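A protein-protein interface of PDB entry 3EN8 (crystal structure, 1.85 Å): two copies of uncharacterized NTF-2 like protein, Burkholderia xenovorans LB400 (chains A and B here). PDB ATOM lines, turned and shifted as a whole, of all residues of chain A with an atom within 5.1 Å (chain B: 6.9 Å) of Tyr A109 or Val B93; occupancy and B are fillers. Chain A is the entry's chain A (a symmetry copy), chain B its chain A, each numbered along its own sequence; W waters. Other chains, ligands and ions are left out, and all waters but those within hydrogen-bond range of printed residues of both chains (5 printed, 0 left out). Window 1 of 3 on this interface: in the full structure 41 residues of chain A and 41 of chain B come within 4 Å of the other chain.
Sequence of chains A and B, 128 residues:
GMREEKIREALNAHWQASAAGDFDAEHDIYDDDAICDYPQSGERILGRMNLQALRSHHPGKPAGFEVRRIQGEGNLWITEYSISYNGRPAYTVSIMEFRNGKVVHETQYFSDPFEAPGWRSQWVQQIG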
ATOM      1  N   PRO A  39      24.507 -27.804 -27.529  1.00  0.00           N
ATOM      2  CA  PRO A  39      23.272 -28.417 -27.007  1.00  0.00           C
ATOM      3  C   PRO A  39      22.308 -28.813 -28.107  1.00  0.00           C
ATOM      4  O   PRO A  39      21.493 -29.698 -27.921  1.00  0.00           O
ATOM      5  CB  PRO A  39      22.719 -27.320 -26.076  1.00  0.00           C
ATOM      6  CG  PRO A  39      23.961 -26.674 -25.537  1.00  0.00           C
ATOM      7  CD  PRO A  39      24.879 -26.600 -26.767  1.00  0.00           C
ATOM      8  N   GLN A  40      22.426 -28.194 -29.269  1.00  0.00           N
ATOM      9  CA  GLN A  40      21.460 -28.448 -30.354  1.00  0.00           C
ATOM     10  C   GLN A  40      21.568 -29.877 -30.847  1.00  0.00           C
ATOM     11  O   GLN A  40      20.609 -30.472 -31.384  1.00  0.00           O
ATOM     12  CB  GLN A  40      21.659 -27.502 -31.536  1.00  0.00           C
ATOM     13  CG  GLN A  40      21.205 -26.081 -31.283  1.00  0.00           C
ATOM     14  CD  GLN A  40      21.821 -25.119 -32.286  1.00  0.00           C
ATOM     15  OE1 GLN A  40      22.891 -24.520 -32.058  1.00  0.00           O
ATOM     16  NE2 GLN A  40      21.164 -24.981 -33.407  1.00  0.00           N
ATOM     17  N   ILE A  78      29.644 -13.903 -22.525  1.00  0.00           N
ATOM     18  CA  ILE A  78      28.806 -14.270 -23.650  1.00  0.00           C
ATOM     19  C   ILE A  78      28.982 -13.371 -24.858  1.00  0.00           C
ATOM     20  O   ILE A  78      28.851 -12.151 -24.811  1.00  0.00           O
ATOM     21  CB  ILE A  78      27.327 -14.423 -23.247  1.00  0.00           C
ATOM     22  CG1 ILE A  78      26.555 -15.025 -24.421  1.00  0.00           C
ATOM     23  CG2 ILE A  78      26.703 -13.102 -22.738  1.00  0.00           C
ATOM     24  CD1 ILE A  78      25.130 -15.404 -24.054  1.00  0.00           C
ATOM     25  N   TYR A  91      23.655 -16.801 -36.853  1.00  0.00           N
ATOM     26  CA  TYR A  91      23.645 -16.008 -35.616  1.00  0.00           C
ATOM     27  C   TYR A  91      24.061 -16.938 -34.497  1.00  0.00           C
ATOM     28  O   TYR A  91      23.324 -17.876 -34.111  1.00  0.00           O
ATOM     29  CB  TYR A  91      22.244 -15.416 -35.350  1.00  0.00           C
ATOM     30  CG  TYR A  91      21.889 -14.254 -36.216  1.00  0.00           C
ATOM     31  CD1 TYR A  91      22.219 -12.959 -35.848  1.00  0.00           C
ATOM     32  CD2 TYR A  91      21.214 -14.450 -37.430  1.00  0.00           C
ATOM     33  CE1 TYR A  91      21.896 -11.871 -36.665  1.00  0.00           C
ATOM     34  CE2 TYR A  91      20.879 -13.370 -38.250  1.00  0.00           C
ATOM     35  CZ  TYR A  91      21.228 -12.083 -37.868  1.00  0.00           C
ATOM     36  OH  TYR A  91      20.914 -11.001 -38.666  1.00  0.00           O
ATOM     37  N   THR A  92      25.253 -16.657 -33.976  1.00  0.00           N
ATOM     38  CA  THR A  92      25.953 -17.540 -33.064  1.00  0.00           C
ATOM     39  C   THR A  92      26.074 -16.904 -31.676  1.00  0.00           C
ATOM     40  O   THR A  92      26.123 -15.689 -31.488  1.00  0.00           O
ATOM     41  CB  THR A  92      27.329 -17.964 -33.663  1.00  0.00           C
ATOM     42  OG1 THR A  92      27.145 -18.440 -35.008  1.00  0.00           O
ATOM     43  CG2 THR A  92      27.959 -19.093 -32.826  1.00  0.00           C
ATOM     44  N   VAL A  93      26.011 -17.776 -30.712  1.00  0.00           N
ATOM     45  CA  VAL A  93      26.193 -17.426 -29.289  1.00  0.00           C
ATOM     46  C   VAL A  93      27.211 -18.349 -28.691  1.00  0.00           C
ATOM     47  O   VAL A  93      27.117 -19.554 -28.794  1.00  0.00           O
ATOM     48  CB  VAL A  93      24.873 -17.518 -28.480  1.00  0.00           C
ATOM     49  CG1 VAL A  93      25.150 -17.280 -26.968  1.00  0.00           C
ATOM     50  CG2 VAL A  93      23.836 -16.509 -28.986  1.00  0.00           C
ATOM     51  N   ILE A  95      28.828 -18.997 -25.024  1.00  0.00           N
ATOM     52  CA  ILE A  95      28.766 -18.780 -23.577  1.00  0.00           C
ATOM     53  C   ILE A  95      30.026 -19.370 -22.990  1.00  0.00           C
ATOM     54  O   ILE A  95      30.256 -20.581 -23.128  1.00  0.00           O
ATOM     55  CB  ILE A  95      27.524 -19.464 -22.935  1.00  0.00           C
ATOM     56  CG1 ILE A  95      26.232 -19.091 -23.615  1.00  0.00           C
ATOM     57  CG2 ILE A  95      27.513 -19.207 -21.412  1.00  0.00           C
ATOM     58  CD1 ILE A  95      25.126 -20.145 -23.378  1.00  0.00           C
ATOM     59  N   THR A 107      29.807 -23.117 -24.339  1.00  0.00           N
ATOM     60  CA  THR A 107      28.588 -23.660 -24.951  1.00  0.00           C
ATOM     61  C   THR A 107      28.235 -22.774 -26.130  1.00  0.00           C
ATOM     62  O   THR A 107      28.077 -21.547 -25.988  1.00  0.00           O
ATOM     63  CB  THR A 107      27.431 -23.607 -23.960  1.00  0.00           C
ATOM     64  OG1 THR A 107      27.858 -24.123 -22.704  1.00  0.00           O
ATOM     65  CG2 THR A 107      26.205 -24.411 -24.483  1.00  0.00           C
ATOM     66  N   GLN A 108      28.078 -23.401 -27.277  1.00  0.00           N
ATOM     67  CA  GLN A 108      27.740 -22.690 -28.487  1.00  0.00           C
ATOM     68  C   GLN A 108      26.379 -23.089 -29.076  1.00  0.00           C
ATOM     69  O   GLN A 108      25.988 -24.251 -29.085  1.00  0.00           O
ATOM     70  CB  GLN A 108      28.826 -22.884 -29.543  1.00  0.00           C
ATOM     71  CG  GLN A 108      30.118 -22.097 -29.338  1.00  0.00           C
ATOM     72  CD  GLN A 108      31.179 -22.455 -30.401  1.00  0.00           C
ATOM     73  OE1 GLN A 108      31.637 -23.585 -30.475  1.00  0.00           O
ATOM     74  NE2 GLN A 108      31.597 -21.465 -31.191  1.00  0.00           N
ATOM     75  N   TYR A 109      25.698 -22.062 -29.560  1.00  0.00           N
ATOM     76  CA  TYR A 109      24.471 -22.189 -30.336  1.00  0.00           C
ATOM     77  C   TYR A 109      24.611 -21.477 -31.694  1.00  0.00           C
ATOM     78  O   TYR A 109      25.143 -20.378 -31.789  1.00  0.00           O
ATOM     79  CB  TYR A 109      23.346 -21.504 -29.593  1.00  0.00           C
ATOM     80  CG  TYR A 109      22.903 -22.225 -28.344  1.00  0.00           C
ATOM     81  CD1 TYR A 109      23.517 -22.009 -27.148  1.00  0.00           C
ATOM     82  CD2 TYR A 109      21.877 -23.178 -28.399  1.00  0.00           C
ATOM     83  CE1 TYR A 109      23.111 -22.673 -25.990  1.00  0.00           C
ATOM     84  CE2 TYR A 109      21.441 -23.820 -27.250  1.00  0.00           C
ATOM     85  CZ  TYR A 109      22.059 -23.578 -26.069  1.00  0.00           C
ATOM     86  OH  TYR A 109      21.636 -24.244 -24.972  1.00  0.00           O
ATOM     87  N   PHE A 110      24.030 -22.089 -32.688  1.00  0.00           N
ATOM     88  CA  PHE A 110      24.120 -21.647 -34.074  1.00  0.00           C
ATOM     89  C   PHE A 110      22.724 -21.554 -34.621  1.00  0.00           C
ATOM     90  O   PHE A 110      22.054 -22.564 -34.784  1.00  0.00           O
ATOM     91  CB  PHE A 110      24.942 -22.638 -34.903  1.00  0.00           C
ATOM     92  CG  PHE A 110      26.295 -22.958 -34.311  1.00  0.00           C
ATOM     93  CD1 PHE A 110      27.392 -22.166 -34.609  1.00  0.00           C
ATOM     94  CD2 PHE A 110      26.467 -24.056 -33.459  1.00  0.00           C
ATOM     95  CE1 PHE A 110      28.643 -22.461 -34.080  1.00  0.00           C
ATOM     96  CE2 PHE A 110      27.737 -24.341 -32.911  1.00  0.00           C
ATOM     97  CZ  PHE A 110      28.798 -23.544 -33.228  1.00  0.00           C
ATOM     98  N   SER A 111      22.268 -20.325 -34.818  1.00  0.00           N
ATOM     99  CA  SER A 111      20.878 -20.071 -35.163  1.00  0.00           C
ATOM    100  C   SER A 111      20.743 -19.420 -36.543  1.00  0.00           C
ATOM    101  O   SER A 111      21.649 -18.735 -37.032  1.00  0.00           O
ATOM    102  CB  SER A 111      20.194 -19.255 -34.047  1.00  0.00           C
ATOM    103  OG  SER A 111      20.507 -17.901 -34.115  1.00  0.00           O
ATOM    104  N   TRP B  15      10.459 -18.535 -15.189  1.00  0.00           N
ATOM    105  CA  TRP B  15      10.396 -19.619 -16.164  1.00  0.00           C
ATOM    106  C   TRP B  15       9.225 -20.536 -15.856  1.00  0.00           C
ATOM    107  O   TRP B  15       8.601 -21.096 -16.755  1.00  0.00           O
ATOM    108  CB  TRP B  15      11.698 -20.427 -16.228  1.00  0.00           C
ATOM    109  CG  TRP B  15      12.832 -19.569 -16.731  1.00  0.00           C
ATOM    110  CD1 TRP B  15      13.985 -19.338 -16.095  1.00  0.00           C
ATOM    111  CD2 TRP B  15      12.861 -18.785 -17.945  1.00  0.00           C
ATOM    112  NE1 TRP B  15      14.774 -18.451 -16.831  1.00  0.00           N
ATOM    113  CE2 TRP B  15      14.100 -18.111 -17.974  1.00  0.00           C
ATOM    114  CE3 TRP B  15      11.958 -18.589 -19.014  1.00  0.00           C
ATOM    115  CZ2 TRP B  15      14.455 -17.244 -19.004  1.00  0.00           C
ATOM    116  CZ3 TRP B  15      12.325 -17.765 -20.032  1.00  0.00           C
ATOM    117  CH2 TRP B  15      13.555 -17.077 -20.007  1.00  0.00           C
ATOM    118  N   ARG B  68      17.163 -25.935 -19.254  1.00  0.00           N
ATOM    119  CA  ARG B  68      18.396 -26.737 -19.377  1.00  0.00           C
ATOM    120  C   ARG B  68      19.441 -26.320 -18.336  1.00  0.00           C
ATOM    121  O   ARG B  68      20.022 -27.105 -17.566  1.00  0.00           O
ATOM    122  CB  ARG B  68      19.012 -26.564 -20.773  1.00  0.00           C
ATOM    123  CG  ARG B  68      20.256 -27.415 -20.974  1.00  0.00           C
ATOM    124  CD  ARG B  68      20.940 -27.195 -22.324  1.00  0.00           C
ATOM    125  NE  ARG B  68      22.157 -28.012 -22.485  1.00  0.00           N
ATOM    126  CZ  ARG B  68      22.171 -29.232 -23.025  1.00  0.00           C
ATOM    127  NH1 ARG B  68      21.051 -29.816 -23.419  1.00  0.00           N
ATOM    128  NH2 ARG B  68      23.317 -29.898 -23.139  1.00  0.00           N
ATOM    129  N   ILE B  78      22.008 -15.800 -17.956  1.00  0.00           N
ATOM    130  CA  ILE B  78      21.717 -16.531 -19.174  1.00  0.00           C
ATOM    131  C   ILE B  78      21.075 -17.884 -18.933  1.00  0.00           C
ATOM    132  O   ILE B  78      21.575 -18.744 -18.214  1.00  0.00           O
ATOM    133  CB  ILE B  78      22.943 -16.624 -20.103  1.00  0.00           C
ATOM    134  CG1 ILE B  78      22.501 -17.203 -21.447  1.00  0.00           C
ATOM    135  CG2 ILE B  78      24.116 -17.411 -19.472  1.00  0.00           C
ATOM    136  CD1 ILE B  78      23.596 -17.146 -22.499  1.00  0.00           C
ATOM    137  N   THR B  79      19.933 -18.019 -19.568  1.00  0.00           N
ATOM    138  CA  THR B  79      19.087 -19.197 -19.418  1.00  0.00           C
ATOM    139  C   THR B  79      19.048 -19.907 -20.755  1.00  0.00           C
ATOM    140  O   THR B  79      18.759 -19.318 -21.803  1.00  0.00           O
ATOM    141  CB  THR B  79      17.640 -18.870 -18.935  1.00  0.00           C
ATOM    142  OG1 THR B  79      17.657 -18.184 -17.691  1.00  0.00           O
ATOM    143  CG2 THR B  79      16.808 -20.174 -18.824  1.00  0.00           C
ATOM    144  N   GLU B  80      19.373 -21.187 -20.674  1.00  0.00           N
ATOM    145  CA  GLU B  80      19.261 -22.114 -21.773  1.00  0.00           C
ATOM    146  C   GLU B  80      18.063 -22.982 -21.502  1.00  0.00           C
ATOM    147  O   GLU B  80      17.926 -23.564 -20.425  1.00  0.00           O
ATOM    148  CB  GLU B  80      20.521 -22.992 -21.880  1.00  0.00           C
ATOM    149  CG  GLU B  80      21.842 -22.253 -22.219  1.00  0.00           C
ATOM    150  CD  GLU B  80      23.005 -23.155 -22.026  1.00  0.00           C
ATOM    151  OE1 GLU B  80      23.095 -24.122 -22.809  1.00  0.00           O
ATOM    152  OE2 GLU B  80      23.806 -22.907 -21.083  1.00  0.00           O
ATOM    153  N   TYR B  81      17.190 -23.073 -22.470  1.00  0.00           N
ATOM    154  CA  TYR B  81      15.910 -23.789 -22.227  1.00  0.00           C
ATOM    155  C   TYR B  81      15.343 -24.207 -23.527  1.00  0.00           C
ATOM    156  O   TYR B  81      15.754 -23.734 -24.546  1.00  0.00           O
ATOM    157  CB  TYR B  81      14.897 -22.948 -21.443  1.00  0.00           C
ATOM    158  CG  TYR B  81      14.373 -21.638 -22.060  1.00  0.00           C
ATOM    159  CD1 TYR B  81      15.163 -20.471 -22.085  1.00  0.00           C
ATOM    160  CD2 TYR B  81      13.099 -21.549 -22.565  1.00  0.00           C
ATOM    161  CE1 TYR B  81      14.686 -19.304 -22.616  1.00  0.00           C
ATOM    162  CE2 TYR B  81      12.594 -20.355 -23.093  1.00  0.00           C
ATOM    163  CZ  TYR B  81      13.406 -19.215 -23.120  1.00  0.00           C
ATOM    164  OH  TYR B  81      12.890 -18.025 -23.660  1.00  0.00           O
ATOM    165  N   ALA B  90      12.442 -25.789 -29.925  1.00  0.00           N
ATOM    166  CA  ALA B  90      13.474 -24.787 -30.123  1.00  0.00           C
ATOM    167  C   ALA B  90      14.384 -24.749 -28.917  1.00  0.00           C
ATOM    168  O   ALA B  90      13.937 -24.637 -27.779  1.00  0.00           O
ATOM    169  CB  ALA B  90      12.861 -23.446 -30.360  1.00  0.00           C
ATOM    170  N   TYR B  91      15.667 -24.893 -29.211  1.00  0.00           N
ATOM    171  CA  TYR B  91      16.742 -24.650 -28.239  1.00  0.00           C
ATOM    172  C   TYR B  91      16.913 -23.150 -28.141  1.00  0.00           C
ATOM    173  O   TYR B  91      17.378 -22.475 -29.090  1.00  0.00           O
ATOM    174  CB  TYR B  91      18.056 -25.327 -28.686  1.00  0.00           C
ATOM    175  CG  TYR B  91      18.084 -26.807 -28.499  1.00  0.00           C
ATOM    176  CD1 TYR B  91      18.506 -27.370 -27.305  1.00  0.00           C
ATOM    177  CD2 TYR B  91      17.676 -27.665 -29.532  1.00  0.00           C
ATOM    178  CE1 TYR B  91      18.522 -28.757 -27.125  1.00  0.00           C
ATOM    179  CE2 TYR B  91      17.696 -29.051 -29.366  1.00  0.00           C
ATOM    180  CZ  TYR B  91      18.113 -29.594 -28.160  1.00  0.00           C
ATOM    181  OH  TYR B  91      18.133 -30.961 -27.971  1.00  0.00           O
ATOM    182  N   THR B  92      16.535 -22.638 -26.971  1.00  0.00           N
ATOM    183  CA  THR B  92      16.390 -21.216 -26.732  1.00  0.00           C
ATOM    184  C   THR B  92      17.427 -20.725 -25.718  1.00  0.00           C
ATOM    185  O   THR B  92      17.897 -21.436 -24.830  1.00  0.00           O
ATOM    186  CB  THR B  92      14.925 -20.879 -26.319  1.00  0.00           C
ATOM    187  OG1 THR B  92      14.009 -21.473 -27.257  1.00  0.00           O
ATOM    188  CG2 THR B  92      14.701 -19.355 -26.313  1.00  0.00           C
ATOM    189  N   VAL B  93      17.839 -19.515 -25.958  1.00  0.00           N
ATOM    190  CA  VAL B  93      18.769 -18.784 -25.074  1.00  0.00           C
ATOM    191  C   VAL B  93      18.186 -17.437 -24.769  1.00  0.00           C
ATOM    192  O   VAL B  93      17.807 -16.693 -25.648  1.00  0.00           O
ATOM    193  CB  VAL B  93      20.175 -18.608 -25.705  1.00  0.00           C
ATOM    194  CG1 VAL B  93      21.064 -17.712 -24.797  1.00  0.00           C
ATOM    195  CG2 VAL B  93      20.858 -19.961 -25.933  1.00  0.00           C
ATOM    196  N   SER B  94      18.088 -17.137 -23.482  1.00  0.00           N
ATOM    197  CA  SER B  94      17.683 -15.837 -23.063  1.00  0.00           C
ATOM    198  C   SER B  94      18.812 -15.208 -22.217  1.00  0.00           C
ATOM    199  O   SER B  94      19.134 -15.720 -21.117  1.00  0.00           O
ATOM    200  CB  SER B  94      16.395 -15.918 -22.213  1.00  0.00           C
ATOM    201  OG  SER B  94      16.119 -14.737 -21.470  1.00  0.00           O
ATOM    202  N   ILE B  95      19.319 -14.114 -22.729  1.00  0.00           N
ATOM    203  CA  ILE B  95      20.389 -13.351 -22.085  1.00  0.00           C
ATOM    204  C   ILE B  95      19.738 -12.169 -21.407  1.00  0.00           C
ATOM    205  O   ILE B  95      19.114 -11.341 -22.089  1.00  0.00           O
ATOM    206  CB  ILE B  95      21.448 -12.847 -23.108  1.00  0.00           C
ATOM    207  CG1 ILE B  95      21.991 -13.948 -23.982  1.00  0.00           C
ATOM    208  CG2 ILE B  95      22.546 -12.046 -22.374  1.00  0.00           C
ATOM    209  CD1 ILE B  95      22.573 -13.403 -25.307  1.00  0.00           C
ATOM    210  N   GLU B 106      16.644  -7.928 -22.423  1.00  0.00           N
ATOM    211  CA  GLU B 106      16.667  -9.358 -22.703  1.00  0.00           C
ATOM    212  C   GLU B 106      16.999  -9.508 -24.163  1.00  0.00           C
ATOM    213  O   GLU B 106      16.528  -8.734 -24.965  1.00  0.00           O
ATOM    214  CB  GLU B 106      15.293  -9.978 -22.430  1.00  0.00           C
ATOM    215  CG  GLU B 106      15.227 -11.476 -22.748  1.00  0.00           C
ATOM    216  CD  GLU B 106      13.920 -12.137 -22.302  1.00  0.00           C
ATOM    217  OE1 GLU B 106      12.910 -11.434 -21.999  1.00  0.00           O
ATOM    218  OE2 GLU B 106      13.923 -13.395 -22.276  1.00  0.00           O
ATOM    219  N   THR B 107      17.826 -10.494 -24.481  1.00  0.00           N
ATOM    220  CA  THR B 107      18.081 -10.890 -25.872  1.00  0.00           C
ATOM    221  C   THR B 107      17.813 -12.379 -25.980  1.00  0.00           C
ATOM    222  O   THR B 107      18.397 -13.192 -25.238  1.00  0.00           O
ATOM    223  CB  THR B 107      19.541 -10.647 -26.232  1.00  0.00           C
ATOM    224  OG1 THR B 107      19.924  -9.344 -25.807  1.00  0.00           O
ATOM    225  CG2 THR B 107      19.778 -10.806 -27.762  1.00  0.00           C
ATOM    226  N   GLN B 108      16.964 -12.731 -26.921  1.00  0.00           N
ATOM    227  CA  GLN B 108      16.611 -14.114 -27.144  1.00  0.00           C
ATOM    228  C   GLN B 108      17.021 -14.639 -28.527  1.00  0.00           C
ATOM    229  O   GLN B 108      16.920 -13.956 -29.540  1.00  0.00           O
ATOM    230  CB  GLN B 108      15.111 -14.321 -26.946  1.00  0.00           C
ATOM    231  CG  GLN B 108      14.613 -14.336 -25.503  1.00  0.00           C
ATOM    232  CD  GLN B 108      13.075 -14.443 -25.431  1.00  0.00           C
ATOM    233  OE1 GLN B 108      12.362 -13.560 -25.884  1.00  0.00           O
ATOM    234  NE2 GLN B 108      12.574 -15.514 -24.813  1.00  0.00           N
ATOM    235  N   TYR B 109      17.483 -15.879 -28.499  1.00  0.00           N
ATOM    236  CA  TYR B 109      17.763 -16.674 -29.688  1.00  0.00           C
ATOM    237  C   TYR B 109      16.987 -18.003 -29.648  1.00  0.00           C
ATOM    238  O   TYR B 109      16.905 -18.665 -28.621  1.00  0.00           O
ATOM    239  CB  TYR B 109      19.234 -17.022 -29.713  1.00  0.00           C
ATOM    240  CG  TYR B 109      20.140 -15.850 -30.000  1.00  0.00           C
ATOM    241  CD1 TYR B 109      20.584 -15.038 -29.002  1.00  0.00           C
ATOM    242  CD2 TYR B 109      20.506 -15.540 -31.317  1.00  0.00           C
ATOM    243  CE1 TYR B 109      21.423 -13.953 -29.263  1.00  0.00           C
ATOM    244  CE2 TYR B 109      21.365 -14.486 -31.587  1.00  0.00           C
ATOM    245  CZ  TYR B 109      21.803 -13.700 -30.576  1.00  0.00           C
ATOM    246  OH  TYR B 109      22.612 -12.659 -30.872  1.00  0.00           O
ATOM    247  N   PHE B 110      16.532 -18.399 -30.804  1.00  0.00           N
ATOM    248  CA  PHE B 110      15.689 -19.575 -30.982  1.00  0.00           C
ATOM    249  C   PHE B 110      16.304 -20.426 -32.056  1.00  0.00           C
ATOM    250  O   PHE B 110      16.337 -20.036 -33.214  1.00  0.00           O
ATOM    251  CB  PHE B 110      14.271 -19.162 -31.389  1.00  0.00           C
ATOM    252  CG  PHE B 110      13.645 -18.136 -30.474  1.00  0.00           C
ATOM    253  CD1 PHE B 110      12.947 -18.540 -29.347  1.00  0.00           C
ATOM    254  CD2 PHE B 110      13.751 -16.766 -30.747  1.00  0.00           C
ATOM    255  CE1 PHE B 110      12.355 -17.603 -28.507  1.00  0.00           C
ATOM    256  CE2 PHE B 110      13.162 -15.819 -29.881  1.00  0.00           C
ATOM    257  CZ  PHE B 110      12.479 -16.250 -28.783  1.00  0.00           C
ATOM    258  N   SER B 111      16.865 -21.553 -31.639  1.00  0.00           N
ATOM    259  CA  SER B 111      17.660 -22.385 -32.528  1.00  0.00           C
ATOM    260  C   SER B 111      17.039 -23.772 -32.718  1.00  0.00           C
ATOM    261  O   SER B 111      16.311 -24.283 -31.859  1.00  0.00           O
ATOM    262  CB  SER B 111      19.121 -22.446 -32.034  1.00  0.00           C
ATOM    263  OG  SER B 111      19.284 -23.337 -30.978  1.00  0.00           O
ATOM    264  N   ASP B 112      17.318 -24.349 -33.880  1.00  0.00           N
ATOM    265  CA  ASP B 112      16.852 -25.698 -34.204  1.00  0.00           C
ATOM    266  C   ASP B 112      17.814 -26.783 -33.717  1.00  0.00           C
ATOM    267  O   ASP B 112      19.032 -26.551 -33.640  1.00  0.00           O
ATOM    268  CB  ASP B 112      16.684 -25.867 -35.713  1.00  0.00           C
ATOM    269  CG  ASP B 112      15.577 -25.020 -36.266  1.00  0.00           C
ATOM    270  OD1 ASP B 112      14.424 -25.185 -35.835  1.00  0.00           O
ATOM    271  OD2 ASP B 112      15.865 -24.197 -37.148  1.00  0.00           O
ATOM    272  N   PHE B 114      20.065 -29.969 -34.424  1.00  0.00           N
ATOM    273  CA  PHE B 114      20.743 -30.575 -35.570  1.00  0.00           C
ATOM    274  C   PHE B 114      21.376 -31.893 -35.186  1.00  0.00           C
ATOM    275  O   PHE B 114      21.662 -32.148 -34.027  1.00  0.00           O
ATOM    276  CB  PHE B 114      21.737 -29.625 -36.269  1.00  0.00           C
ATOM    277  CG  PHE B 114      22.946 -29.253 -35.451  1.00  0.00           C
ATOM    278  CD1 PHE B 114      24.048 -30.088 -35.409  1.00  0.00           C
ATOM    279  CD2 PHE B 114      23.001 -28.052 -34.768  1.00  0.00           C
ATOM    280  CE1 PHE B 114      25.153 -29.753 -34.683  1.00  0.00           C
ATOM    281  CE2 PHE B 114      24.125 -27.712 -34.040  1.00  0.00           C
ATOM    282  CZ  PHE B 114      25.187 -28.576 -33.984  1.00  0.00           C
HETATM  283  O   HOH W   1      24.470 -13.604 -32.788  1.00  0.00           O
HETATM  284  O   HOH W   2      19.119 -23.185 -35.782  1.00  0.00           O
HETATM  285  O   HOH W   3      18.807 -24.244 -25.072  1.00  0.00           O
HETATM  286  O   HOH W   4      19.416 -32.892 -31.528  1.00  0.00           O
HETATM  287  O   HOH W   5      26.008 -24.314 -20.677  1.00  0.00           O
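OG of Ser B111 sits close to NE2 of Gln A40.
The side-chain hydroxyl (OH) of Tyr A109 sits at hydrogen-bond distance from the side-chain carboxylate (OE1) of Glu B80 (2.6 Å).
The backbone carbonyl oxygen (O) of Gln A40 is in hydrogen-bond range of the backbone NH (N) of Phe B114.
The side-chain amide nitrogen (NE2) of Gln A40 is in hydrogen-bond range of the backbone carbonyl oxygen (O) of Asp B112 (2.7 Å).
The backbone NH (N) of Ile A95 is in hydrogen-bond range of the backbone carbonyl oxygen (O) of Thr A107 (2.8 Å).
The backbone carbonyl oxygen (O) of Tyr B91 lies within hydrogen-bond range of the backbone NH (N) of Ser B111 (2.8 Å).
The backbone NH of Phe A110 is in hydrogen-bond range of the side-chain amide oxygen of Gln A40 (2.8 Å).
The backbone carbonyl oxygen of Tyr B109 sits at hydrogen-bond distance from the backbone NH of Val B93 (2.9 Å).
The backbone carbonyl oxygen (O) of Tyr A109 lies within hydrogen-bond range of the backbone NH (N) of Val A93, 2.9 Å away.
N of Ser A111 lies within hydrogen-bond range of O of Tyr A91 (2.8 Å).
Among the printed residues, merely in contact across the chains: Pro A39 with Arg B68 (3.6 Å), Pro A39 with Glu B80 (3.8 Å), Pro A39 with Tyr B91 (3.2 Å), Gln A40 with Tyr B91 (3.8 Å), Ile A78 with Ile B78 (2.8 Å), Ile A78 with Ile B95 (3.5 Å), Tyr A91 with Tyr B109 (3.97 Å), Val A93 with Tyr B109 (3.5 Å), Ile A95 with Ile B78 (3.5 Å), Ile A95 with Glu B80 (3.8 Å), Thr A107 with Glu B80 (3.5 Å), Tyr A109 with Tyr B91 (3.97 Å), Tyr A109 with Val B93 (3.5 Å), Tyr A109 with Ser B111 (3.7 Å), Ser A111 with Tyr B109 (3.7 Å) and Ser A111 with Ser B111 (3.9 Å).
Of the printed residues of chain B, Pro A39 touches Arg B68 (3.6 Å), Glu B80 (3.8 Å) and Tyr B91 (3.2 Å).
Of the printed residues of chain B, Ile A95 touches Ile B78 (3.5 Å) and Glu B80 (3.8 Å).
Tyr A109 touches just these residues of chain B: Glu B80 (2.6 Å), Tyr B91 (3.97 Å), Val B93 (3.5 Å) and Ser B111 (3.7 Å).
Of the printed residues of chain B, Ser A111 touches Tyr B109 (3.7 Å) and Ser B111 (3.9 Å).
Trp B15 touches none of the printed residues of chain A.
Of the printed residues of chain A, Val B93 touches Tyr A109.
Of the printed residues of chain A, Tyr B109 touches Tyr A91, Val A93 and Ser A111.
The nearest residue of chain B that does not touch Tyr A109 is Arg B68 (4.03 Å).
The nearest residue of chain A that does not touch Val B93 is Val A93 (4.6 Å).
Hydrophobic or aromatic side chains of chain A that line the printed part of chain B: Pro A39, Ile A78, Tyr A91, Val A93, Ile A95 and Tyr A109.
Printed residues of chain B that touch a printed residue of chain A: Arg B68, Ile B78, Glu B80, Tyr B91, Val B93, Ile B95, Tyr B109, Ser B111, Asp B112 and Phe B114.
Tyr A91 touches Tyr B109, and with the chains exchanged Tyr A109 touches Tyr B91.
Val A93 touches Tyr B109, and with the chains exchanged Tyr A109 touches Val B93.
Tyr A109 touches Ser B111, and with the chains exchanged Ser A111 touches Tyr B109.
Ser A111 touches its own counterpart, Ser B111.
Positions printed for both chains: 78, 91, 92, 93, 95, 107, 108, 109, 110 and 111.
Water W5 bridges OE2 of Glu B80 (2.6 Å) and OG1 of Thr A107 (2.8 Å).
Water W4 lies within hydrogen-bond range of O of Gln A40 (2.7 Å) and O of Phe B114 (3.4 Å).
Water W1 lies within hydrogen-bond range of the side-chain hydroxyl (OH) of Tyr B109 and the backbone carbonyl oxygen (O) of Thr A92.
Water W3 lies within hydrogen-bond range of OH of Tyr A109 (2.8 Å), O of Thr B92 (3.0 Å) and O of Tyr B81 (3.1 Å).
Water W2 bridges N of Asp B112 and O of Phe A110.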
